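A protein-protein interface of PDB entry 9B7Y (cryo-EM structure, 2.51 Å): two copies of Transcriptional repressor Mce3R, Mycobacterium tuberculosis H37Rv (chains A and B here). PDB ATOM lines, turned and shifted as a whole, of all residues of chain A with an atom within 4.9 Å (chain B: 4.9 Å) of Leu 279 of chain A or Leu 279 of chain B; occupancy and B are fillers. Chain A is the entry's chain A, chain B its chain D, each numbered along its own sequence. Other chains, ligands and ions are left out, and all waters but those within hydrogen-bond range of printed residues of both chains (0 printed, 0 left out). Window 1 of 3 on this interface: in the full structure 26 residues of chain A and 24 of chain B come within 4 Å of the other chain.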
ATOM      1  N   GLU A 275     -23.586  31.184 -25.754  1.00  0.00           N
ATOM      2  CA  GLU A 275     -24.454  30.060 -25.417  1.00  0.00           C
ATOM      3  C   GLU A 275     -24.972  29.362 -26.667  1.00  0.00           C
ATOM      4  O   GLU A 275     -25.069  28.129 -26.697  1.00  0.00           O
ATOM      5  CB  GLU A 275     -25.616  30.532 -24.543  1.00  0.00           C
ATOM      6  CG  GLU A 275     -25.198  31.068 -23.181  1.00  0.00           C
ATOM      7  CD  GLU A 275     -24.410  30.061 -22.366  1.00  0.00           C
ATOM      8  OE1 GLU A 275     -24.698  28.849 -22.468  1.00  0.00           O
ATOM      9  OE2 GLU A 275     -23.498  30.480 -21.623  1.00  0.00           O
ATOM     10  N   TRP A 276     -25.320  30.126 -27.706  1.00  0.00           N
ATOM     11  CA  TRP A 276     -25.794  29.502 -28.939  1.00  0.00           C
ATOM     12  C   TRP A 276     -24.696  28.668 -29.593  1.00  0.00           C
ATOM     13  O   TRP A 276     -24.946  27.543 -30.052  1.00  0.00           O
ATOM     14  CB  TRP A 276     -26.315  30.570 -29.899  1.00  0.00           C
ATOM     15  CG  TRP A 276     -27.591  31.208 -29.437  1.00  0.00           C
ATOM     16  CD1 TRP A 276     -28.213  31.020 -28.237  1.00  0.00           C
ATOM     17  CD2 TRP A 276     -28.404  32.133 -30.169  1.00  0.00           C
ATOM     18  NE1 TRP A 276     -29.358  31.774 -28.174  1.00  0.00           N
ATOM     19  CE2 TRP A 276     -29.500  32.464 -29.348  1.00  0.00           C
ATOM     20  CE3 TRP A 276     -28.313  32.713 -31.437  1.00  0.00           C
ATOM     21  CZ2 TRP A 276     -30.495  33.348 -29.753  1.00  0.00           C
ATOM     22  CZ3 TRP A 276     -29.304  33.592 -31.838  1.00  0.00           C
ATOM     23  CH2 TRP A 276     -30.379  33.901 -30.998  1.00  0.00           C
ATOM     24  N   ARG A 277     -23.469  29.199 -29.635  1.00  0.00           N
ATOM     25  CA  ARG A 277     -22.349  28.428 -30.168  1.00  0.00           C
ATOM     26  C   ARG A 277     -22.114  27.164 -29.353  1.00  0.00           C
ATOM     27  O   ARG A 277     -21.854  26.094 -29.917  1.00  0.00           O
ATOM     28  CB  ARG A 277     -21.081  29.282 -30.200  1.00  0.00           C
ATOM     29  CG  ARG A 277     -21.167  30.527 -31.065  1.00  0.00           C
ATOM     30  CD  ARG A 277     -20.877  30.215 -32.523  1.00  0.00           C
ATOM     31  NE  ARG A 277     -20.376  31.389 -33.228  1.00  0.00           N
ATOM     32  CZ  ARG A 277     -20.589  31.641 -34.511  1.00  0.00           C
ATOM     33  NH1 ARG A 277     -21.261  30.800 -35.280  1.00  0.00           N
ATOM     34  NH2 ARG A 277     -20.111  32.764 -35.040  1.00  0.00           N
ATOM     35  N   CYS A 278     -22.196  27.267 -28.024  1.00  0.00           N
ATOM     36  CA  CYS A 278     -21.994  26.096 -27.177  1.00  0.00           C
ATOM     37  C   CYS A 278     -23.061  25.038 -27.432  1.00  0.00           C
ATOM     38  O   CYS A 278     -22.756  23.841 -27.500  1.00  0.00           O
ATOM     39  CB  CYS A 278     -21.987  26.511 -25.706  1.00  0.00           C
ATOM     40  SG  CYS A 278     -22.108  25.137 -24.541  1.00  0.00           S
ATOM     41  N   LEU A 279     -24.321  25.461 -27.569  1.00  0.00           N
ATOM     42  CA  LEU A 279     -25.394  24.507 -27.834  1.00  0.00           C
ATOM     43  C   LEU A 279     -25.194  23.811 -29.173  1.00  0.00           C
ATOM     44  O   LEU A 279     -25.369  22.589 -29.281  1.00  0.00           O
ATOM     45  CB  LEU A 279     -26.749  25.215 -27.796  1.00  0.00           C
ATOM     46  CG  LEU A 279     -27.955  24.405 -28.282  1.00  0.00           C
ATOM     47  CD1 LEU A 279     -28.159  23.165 -27.426  1.00  0.00           C
ATOM     48  CD2 LEU A 279     -29.210  25.261 -28.293  1.00  0.00           C
ATOM     49  N   GLU A 280     -24.825  24.569 -30.208  1.00  0.00           N
ATOM     50  CA  GLU A 280     -24.596  23.952 -31.511  1.00  0.00           C
ATOM     51  C   GLU A 280     -23.410  22.995 -31.474  1.00  0.00           C
ATOM     52  O   GLU A 280     -23.451  21.923 -32.087  1.00  0.00           O
ATOM     53  CB  GLU A 280     -24.399  25.023 -32.580  1.00  0.00           C
ATOM     54  CG  GLU A 280     -25.704  25.553 -33.138  1.00  0.00           C
ATOM     55  CD  GLU A 280     -26.488  24.497 -33.892  1.00  0.00           C
ATOM     56  OE1 GLU A 280     -25.861  23.583 -34.468  1.00  0.00           O
ATOM     57  OE2 GLU A 280     -27.733  24.582 -33.910  1.00  0.00           O
ATOM     58  N   CYS A 281     -22.344  23.365 -30.758  1.00  0.00           N
ATOM     59  CA  CYS A 281     -21.198  22.471 -30.628  1.00  0.00           C
ATOM     60  C   CYS A 281     -21.579  21.184 -29.910  1.00  0.00           C
ATOM     61  O   CYS A 281     -21.156  20.093 -30.310  1.00  0.00           O
ATOM     62  CB  CYS A 281     -20.062  23.179 -29.890  1.00  0.00           C
ATOM     63  SG  CYS A 281     -18.598  22.154 -29.615  1.00  0.00           S
ATOM     64  N   ILE A 282     -22.379  21.290 -28.847  1.00  0.00           N
ATOM     65  CA  ILE A 282     -22.815  20.102 -28.118  1.00  0.00           C
ATOM     66  C   ILE A 282     -23.654  19.203 -29.017  1.00  0.00           C
ATOM     67  O   ILE A 282     -23.472  17.978 -29.042  1.00  0.00           O
ATOM     68  CB  ILE A 282     -23.581  20.510 -26.845  1.00  0.00           C
ATOM     69  CG1 ILE A 282     -22.601  20.926 -25.748  1.00  0.00           C
ATOM     70  CG2 ILE A 282     -24.473  19.377 -26.362  1.00  0.00           C
ATOM     71  CD1 ILE A 282     -23.270  21.493 -24.518  1.00  0.00           C
ATOM     72  N   ARG A 283     -24.586  19.794 -29.771  1.00  0.00           N
ATOM     73  CA  ARG A 283     -25.419  18.996 -30.666  1.00  0.00           C
ATOM     74  C   ARG A 283     -24.584  18.315 -31.744  1.00  0.00           C
ATOM     75  O   ARG A 283     -24.806  17.139 -32.061  1.00  0.00           O
ATOM     76  CB  ARG A 283     -26.503  19.869 -31.297  1.00  0.00           C
ATOM     77  CG  ARG A 283     -27.559  20.346 -30.318  1.00  0.00           C
ATOM     78  CD  ARG A 283     -28.903  20.515 -31.004  1.00  0.00           C
ATOM     79  NE  ARG A 283     -29.700  21.571 -30.392  1.00  0.00           N
ATOM     80  CZ  ARG A 283     -30.999  21.739 -30.591  1.00  0.00           C
ATOM     81  NH1 ARG A 283     -31.685  20.939 -31.390  1.00  0.00           N
ATOM     82  NH2 ARG A 283     -31.626  22.736 -29.975  1.00  0.00           N
ATOM     83  N   ILE A 305     -25.142  29.136 -37.287  1.00  0.00           N
ATOM     84  CA  ILE A 305     -25.253  30.206 -36.300  1.00  0.00           C
ATOM     85  C   ILE A 305     -24.791  31.533 -36.893  1.00  0.00           C
ATOM     86  O   ILE A 305     -25.427  32.574 -36.684  1.00  0.00           O
ATOM     87  CB  ILE A 305     -24.472  29.851 -35.023  1.00  0.00           C
ATOM     88  CG1 ILE A 305     -25.218  28.781 -34.236  1.00  0.00           C
ATOM     89  CG2 ILE A 305     -24.290  31.081 -34.148  1.00  0.00           C
ATOM     90  CD1 ILE A 305     -26.592  29.210 -33.771  1.00  0.00           C
ATOM     91  N   GLU B 275     -30.895  31.065 -22.466  1.00  0.00           N
ATOM     92  CA  GLU B 275     -30.494  31.359 -23.838  1.00  0.00           C
ATOM     93  C   GLU B 275     -30.888  30.235 -24.789  1.00  0.00           C
ATOM     94  O   GLU B 275     -31.292  30.497 -25.927  1.00  0.00           O
ATOM     95  CB  GLU B 275     -28.989  31.624 -23.908  1.00  0.00           C
ATOM     96  CG  GLU B 275     -28.515  32.785 -23.045  1.00  0.00           C
ATOM     97  CD  GLU B 275     -28.836  34.146 -23.639  1.00  0.00           C
ATOM     98  OE1 GLU B 275     -29.467  34.203 -24.716  1.00  0.00           O
ATOM     99  OE2 GLU B 275     -28.457  35.165 -23.024  1.00  0.00           O
ATOM    100  N   TRP B 276     -30.778  28.978 -24.350  1.00  0.00           N
ATOM    101  CA  TRP B 276     -31.190  27.872 -25.209  1.00  0.00           C
ATOM    102  C   TRP B 276     -32.689  27.922 -25.486  1.00  0.00           C
ATOM    103  O   TRP B 276     -33.128  27.729 -26.630  1.00  0.00           O
ATOM    104  CB  TRP B 276     -30.804  26.539 -24.571  1.00  0.00           C
ATOM    105  CG  TRP B 276     -29.327  26.284 -24.564  1.00  0.00           C
ATOM    106  CD1 TRP B 276     -28.342  27.153 -24.937  1.00  0.00           C
ATOM    107  CD2 TRP B 276     -28.667  25.077 -24.166  1.00  0.00           C
ATOM    108  NE1 TRP B 276     -27.111  26.563 -24.792  1.00  0.00           N
ATOM    109  CE2 TRP B 276     -27.283  25.289 -24.322  1.00  0.00           C
ATOM    110  CE3 TRP B 276     -29.110  23.839 -23.692  1.00  0.00           C
ATOM    111  CZ2 TRP B 276     -26.340  24.310 -24.022  1.00  0.00           C
ATOM    112  CZ3 TRP B 276     -28.171  22.868 -23.395  1.00  0.00           C
ATOM    113  CH2 TRP B 276     -26.804  23.109 -23.560  1.00  0.00           C
ATOM    114  N   ARG B 277     -33.489  28.193 -24.451  1.00  0.00           N
ATOM    115  CA  ARG B 277     -34.929  28.327 -24.649  1.00  0.00           C
ATOM    116  C   ARG B 277     -35.254  29.497 -25.568  1.00  0.00           C
ATOM    117  O   ARG B 277     -36.149  29.398 -26.415  1.00  0.00           O
ATOM    118  CB  ARG B 277     -35.633  28.484 -23.302  1.00  0.00           C
ATOM    119  CG  ARG B 277     -35.650  27.217 -22.466  1.00  0.00           C
ATOM    120  CD  ARG B 277     -36.991  27.041 -21.774  1.00  0.00           C
ATOM    121  NE  ARG B 277     -36.988  25.912 -20.852  1.00  0.00           N
ATOM    122  CZ  ARG B 277     -37.109  24.644 -21.221  1.00  0.00           C
ATOM    123  NH1 ARG B 277     -37.269  24.307 -22.490  1.00  0.00           N
ATOM    124  NH2 ARG B 277     -37.076  23.692 -20.295  1.00  0.00           N
ATOM    125  N   CYS B 278     -34.538  30.615 -25.416  1.00  0.00           N
ATOM    126  CA  CYS B 278     -34.767  31.762 -26.289  1.00  0.00           C
ATOM    127  C   CYS B 278     -34.446  31.425 -27.740  1.00  0.00           C
ATOM    128  O   CYS B 278     -35.189  31.808 -28.653  1.00  0.00           O
ATOM    129  CB  CYS B 278     -33.935  32.953 -25.817  1.00  0.00           C
ATOM    130  SG  CYS B 278     -34.113  34.437 -26.831  1.00  0.00           S
ATOM    131  N   LEU B 279     -33.340  30.714 -27.975  1.00  0.00           N
ATOM    132  CA  LEU B 279     -32.982  30.333 -29.337  1.00  0.00           C
ATOM    133  C   LEU B 279     -34.030  29.412 -29.945  1.00  0.00           C
ATOM    134  O   LEU B 279     -34.415  29.578 -31.111  1.00  0.00           O
ATOM    135  CB  LEU B 279     -31.608  29.661 -29.353  1.00  0.00           C
ATOM    136  CG  LEU B 279     -31.199  28.973 -30.658  1.00  0.00           C
ATOM    137  CD1 LEU B 279     -31.097  29.979 -31.793  1.00  0.00           C
ATOM    138  CD2 LEU B 279     -29.891  28.221 -30.487  1.00  0.00           C
ATOM    139  N   GLU B 280     -34.505  28.432 -29.172  1.00  0.00           N
ATOM    140  CA  GLU B 280     -35.533  27.535 -29.692  1.00  0.00           C
ATOM    141  C   GLU B 280     -36.831  28.281 -29.977  1.00  0.00           C
ATOM    142  O   GLU B 280     -37.496  28.017 -30.986  1.00  0.00           O
ATOM    143  CB  GLU B 280     -35.771  26.381 -28.721  1.00  0.00           C
ATOM    144  CG  GLU B 280     -34.827  25.213 -28.936  1.00  0.00           C
ATOM    145  CD  GLU B 280     -35.021  24.541 -30.282  1.00  0.00           C
ATOM    146  OE1 GLU B 280     -36.148  24.587 -30.817  1.00  0.00           O
ATOM    147  OE2 GLU B 280     -34.044  23.966 -30.805  1.00  0.00           O
ATOM    148  N   CYS B 281     -37.209  29.216 -29.102  1.00  0.00           N
ATOM    149  CA  CYS B 281     -38.410  30.010 -29.340  1.00  0.00           C
ATOM    150  C   CYS B 281     -38.273  30.852 -30.602  1.00  0.00           C
ATOM    151  O   CYS B 281     -39.220  30.960 -31.388  1.00  0.00           O
ATOM    152  CB  CYS B 281     -38.703  30.897 -28.131  1.00  0.00           C
ATOM    153  SG  CYS B 281     -40.096  32.027 -28.354  1.00  0.00           S
ATOM    154  N   ILE B 282     -37.102  31.458 -30.810  1.00  0.00           N
ATOM    155  CA  ILE B 282     -36.879  32.262 -32.008  1.00  0.00           C
ATOM    156  C   ILE B 282     -36.973  31.396 -33.259  1.00  0.00           C
ATOM    157  O   ILE B 282     -37.602  31.780 -34.254  1.00  0.00           O
ATOM    158  CB  ILE B 282     -35.524  32.990 -31.918  1.00  0.00           C
ATOM    159  CG1 ILE B 282     -35.645  34.230 -31.032  1.00  0.00           C
ATOM    160  CG2 ILE B 282     -35.021  33.373 -33.301  1.00  0.00           C
ATOM    161  CD1 ILE B 282     -34.343  34.974 -30.846  1.00  0.00           C
ATOM    162  N   ARG B 283     -36.353  30.214 -33.229  1.00  0.00           N
ATOM    163  CA  ARG B 283     -36.411  29.324 -34.385  1.00  0.00           C
ATOM    164  C   ARG B 283     -37.840  28.876 -34.670  1.00  0.00           C
ATOM    165  O   ARG B 283     -38.264  28.834 -35.831  1.00  0.00           O
ATOM    166  CB  ARG B 283     -35.501  28.115 -34.166  1.00  0.00           C
ATOM    167  CG  ARG B 283     -34.042  28.378 -34.496  1.00  0.00           C
ATOM    168  CD  ARG B 283     -33.242  27.088 -34.533  1.00  0.00           C
ATOM    169  NE  ARG B 283     -31.837  27.328 -34.839  1.00  0.00           N
ATOM    170  CZ  ARG B 283     -30.837  26.569 -34.412  1.00  0.00           C
ATOM    171  NH1 ARG B 283     -31.050  25.507 -33.655  1.00  0.00           N
ATOM    172  NH2 ARG B 283     -29.591  26.885 -34.755  1.00  0.00           N
ATOM    173  N   ILE B 305     -35.825  20.878 -25.739  1.00  0.00           N
ATOM    174  CA  ILE B 305     -34.866  21.414 -24.775  1.00  0.00           C
ATOM    175  C   ILE B 305     -35.003  20.702 -23.434  1.00  0.00           C
ATOM    176  O   ILE B 305     -34.002  20.354 -22.796  1.00  0.00           O
ATOM    177  CB  ILE B 305     -35.034  22.936 -24.628  1.00  0.00           C
ATOM    178  CG1 ILE B 305     -34.505  23.644 -25.872  1.00  0.00           C
ATOM    179  CG2 ILE B 305     -34.283  23.441 -23.406  1.00  0.00           C
ATOM    180  CD1 ILE B 305     -33.030  23.423 -26.119  1.00  0.00           C
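Leu 279 of chain A touches just these residues of chain B: Trp 276 (3.3 Å) and Leu 279 (3.7 Å). Of the printed residues of chain B, Ile 305 of chain A touches Arg 283. Of the printed residues of chain A, Glu 280 of chain B touches Arg 283. Of the printed residues of chain A, Arg 283 of chain B touches Glu 280 and Ile 305. The nearest residue of chain B that does not touch Leu 279 of chain A is Ile 305 of chain B (4.8 Å). The nearest residue of chain A that does not touch Leu 279 of chain B is Ile 305 of chain A (4.8 Å). The nearest printed residue of chain A that does not touch Trp 276 of chain B is Ile 282 of chain A (4.002 Å).
Glu 275 of chain A touches its own counterpart, Glu 275 of chain B. Trp 276 of chain A touches Leu 279 of chain B, and with the chains exchanged Leu 279 of chain A touches Trp 276 of chain B. Leu 279 of chain A touches its own counterpart, Leu 279 of chain B. Glu 280 of chain A touches Arg 283 of chain B, and with the chains exchanged Arg 283 of chain A touches Glu 280 of chain B. Of the 9 pairs that touch across the chains among the printed residues, 8 have their exchanged pair printed and touching as well.
Among the printed residues, pairs that only touch across the chains: Glu 275 of chain A with Glu 275 of chain B, Trp 276 of chain A with Leu 279 of chain B, Leu 279 of chain A with Trp 276 of chain B, Leu 279 of chain A with Leu 279 of chain B and Ile 305 of chain A with Arg 283 of chain B.
O of Glu 275 of chain B lies within hydrogen-bond range of NE1 of Trp 276 of chain A, at 3.2 Å. The guanidinium group of Arg 283 of chain A lies within salt-bridge range of the side-chain carboxylate of Glu 280 of chain B (2.8 Å). OE2 of Glu 280 of chain A is in salt-bridge range of NH2 of Arg 283 of chain B, 3.1 Å away. O of Glu 275 of chain A is in hydrogen-bond range of NE1 of Trp 276 of chain B (3.2 Å).
Of the 10 printed residues of chain B, 5 touch a printed residue of chain A. Hydrophobic or aromatic side chains of chain B within 4 Å of the printed part of chain A: Trp 276 and Leu 279. Of the 10 printed residues of chain A, 6 touch a printed residue of chain B. Printed residues of chain A that touch a printed residue of chain B: Glu 275, Trp 276, Leu 279, Glu 280, Arg 283 and Ile 305. Hydrophobic or aromatic side chains of chain A within 4 Å of the printed part of chain B: Trp 276, Leu 279 and Ile 305. Among the printed residues, 9 pairs touch across the chains. Among the printed residues, Asp or Glu carboxylates within 4 Å of a Lys or Arg side-chain nitrogen of the other chain: Glu 280 of chain A with Arg 283 of chain B (3.1 Å) and Arg 283 of chain A with Glu 280 of chain B (2.8 Å).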
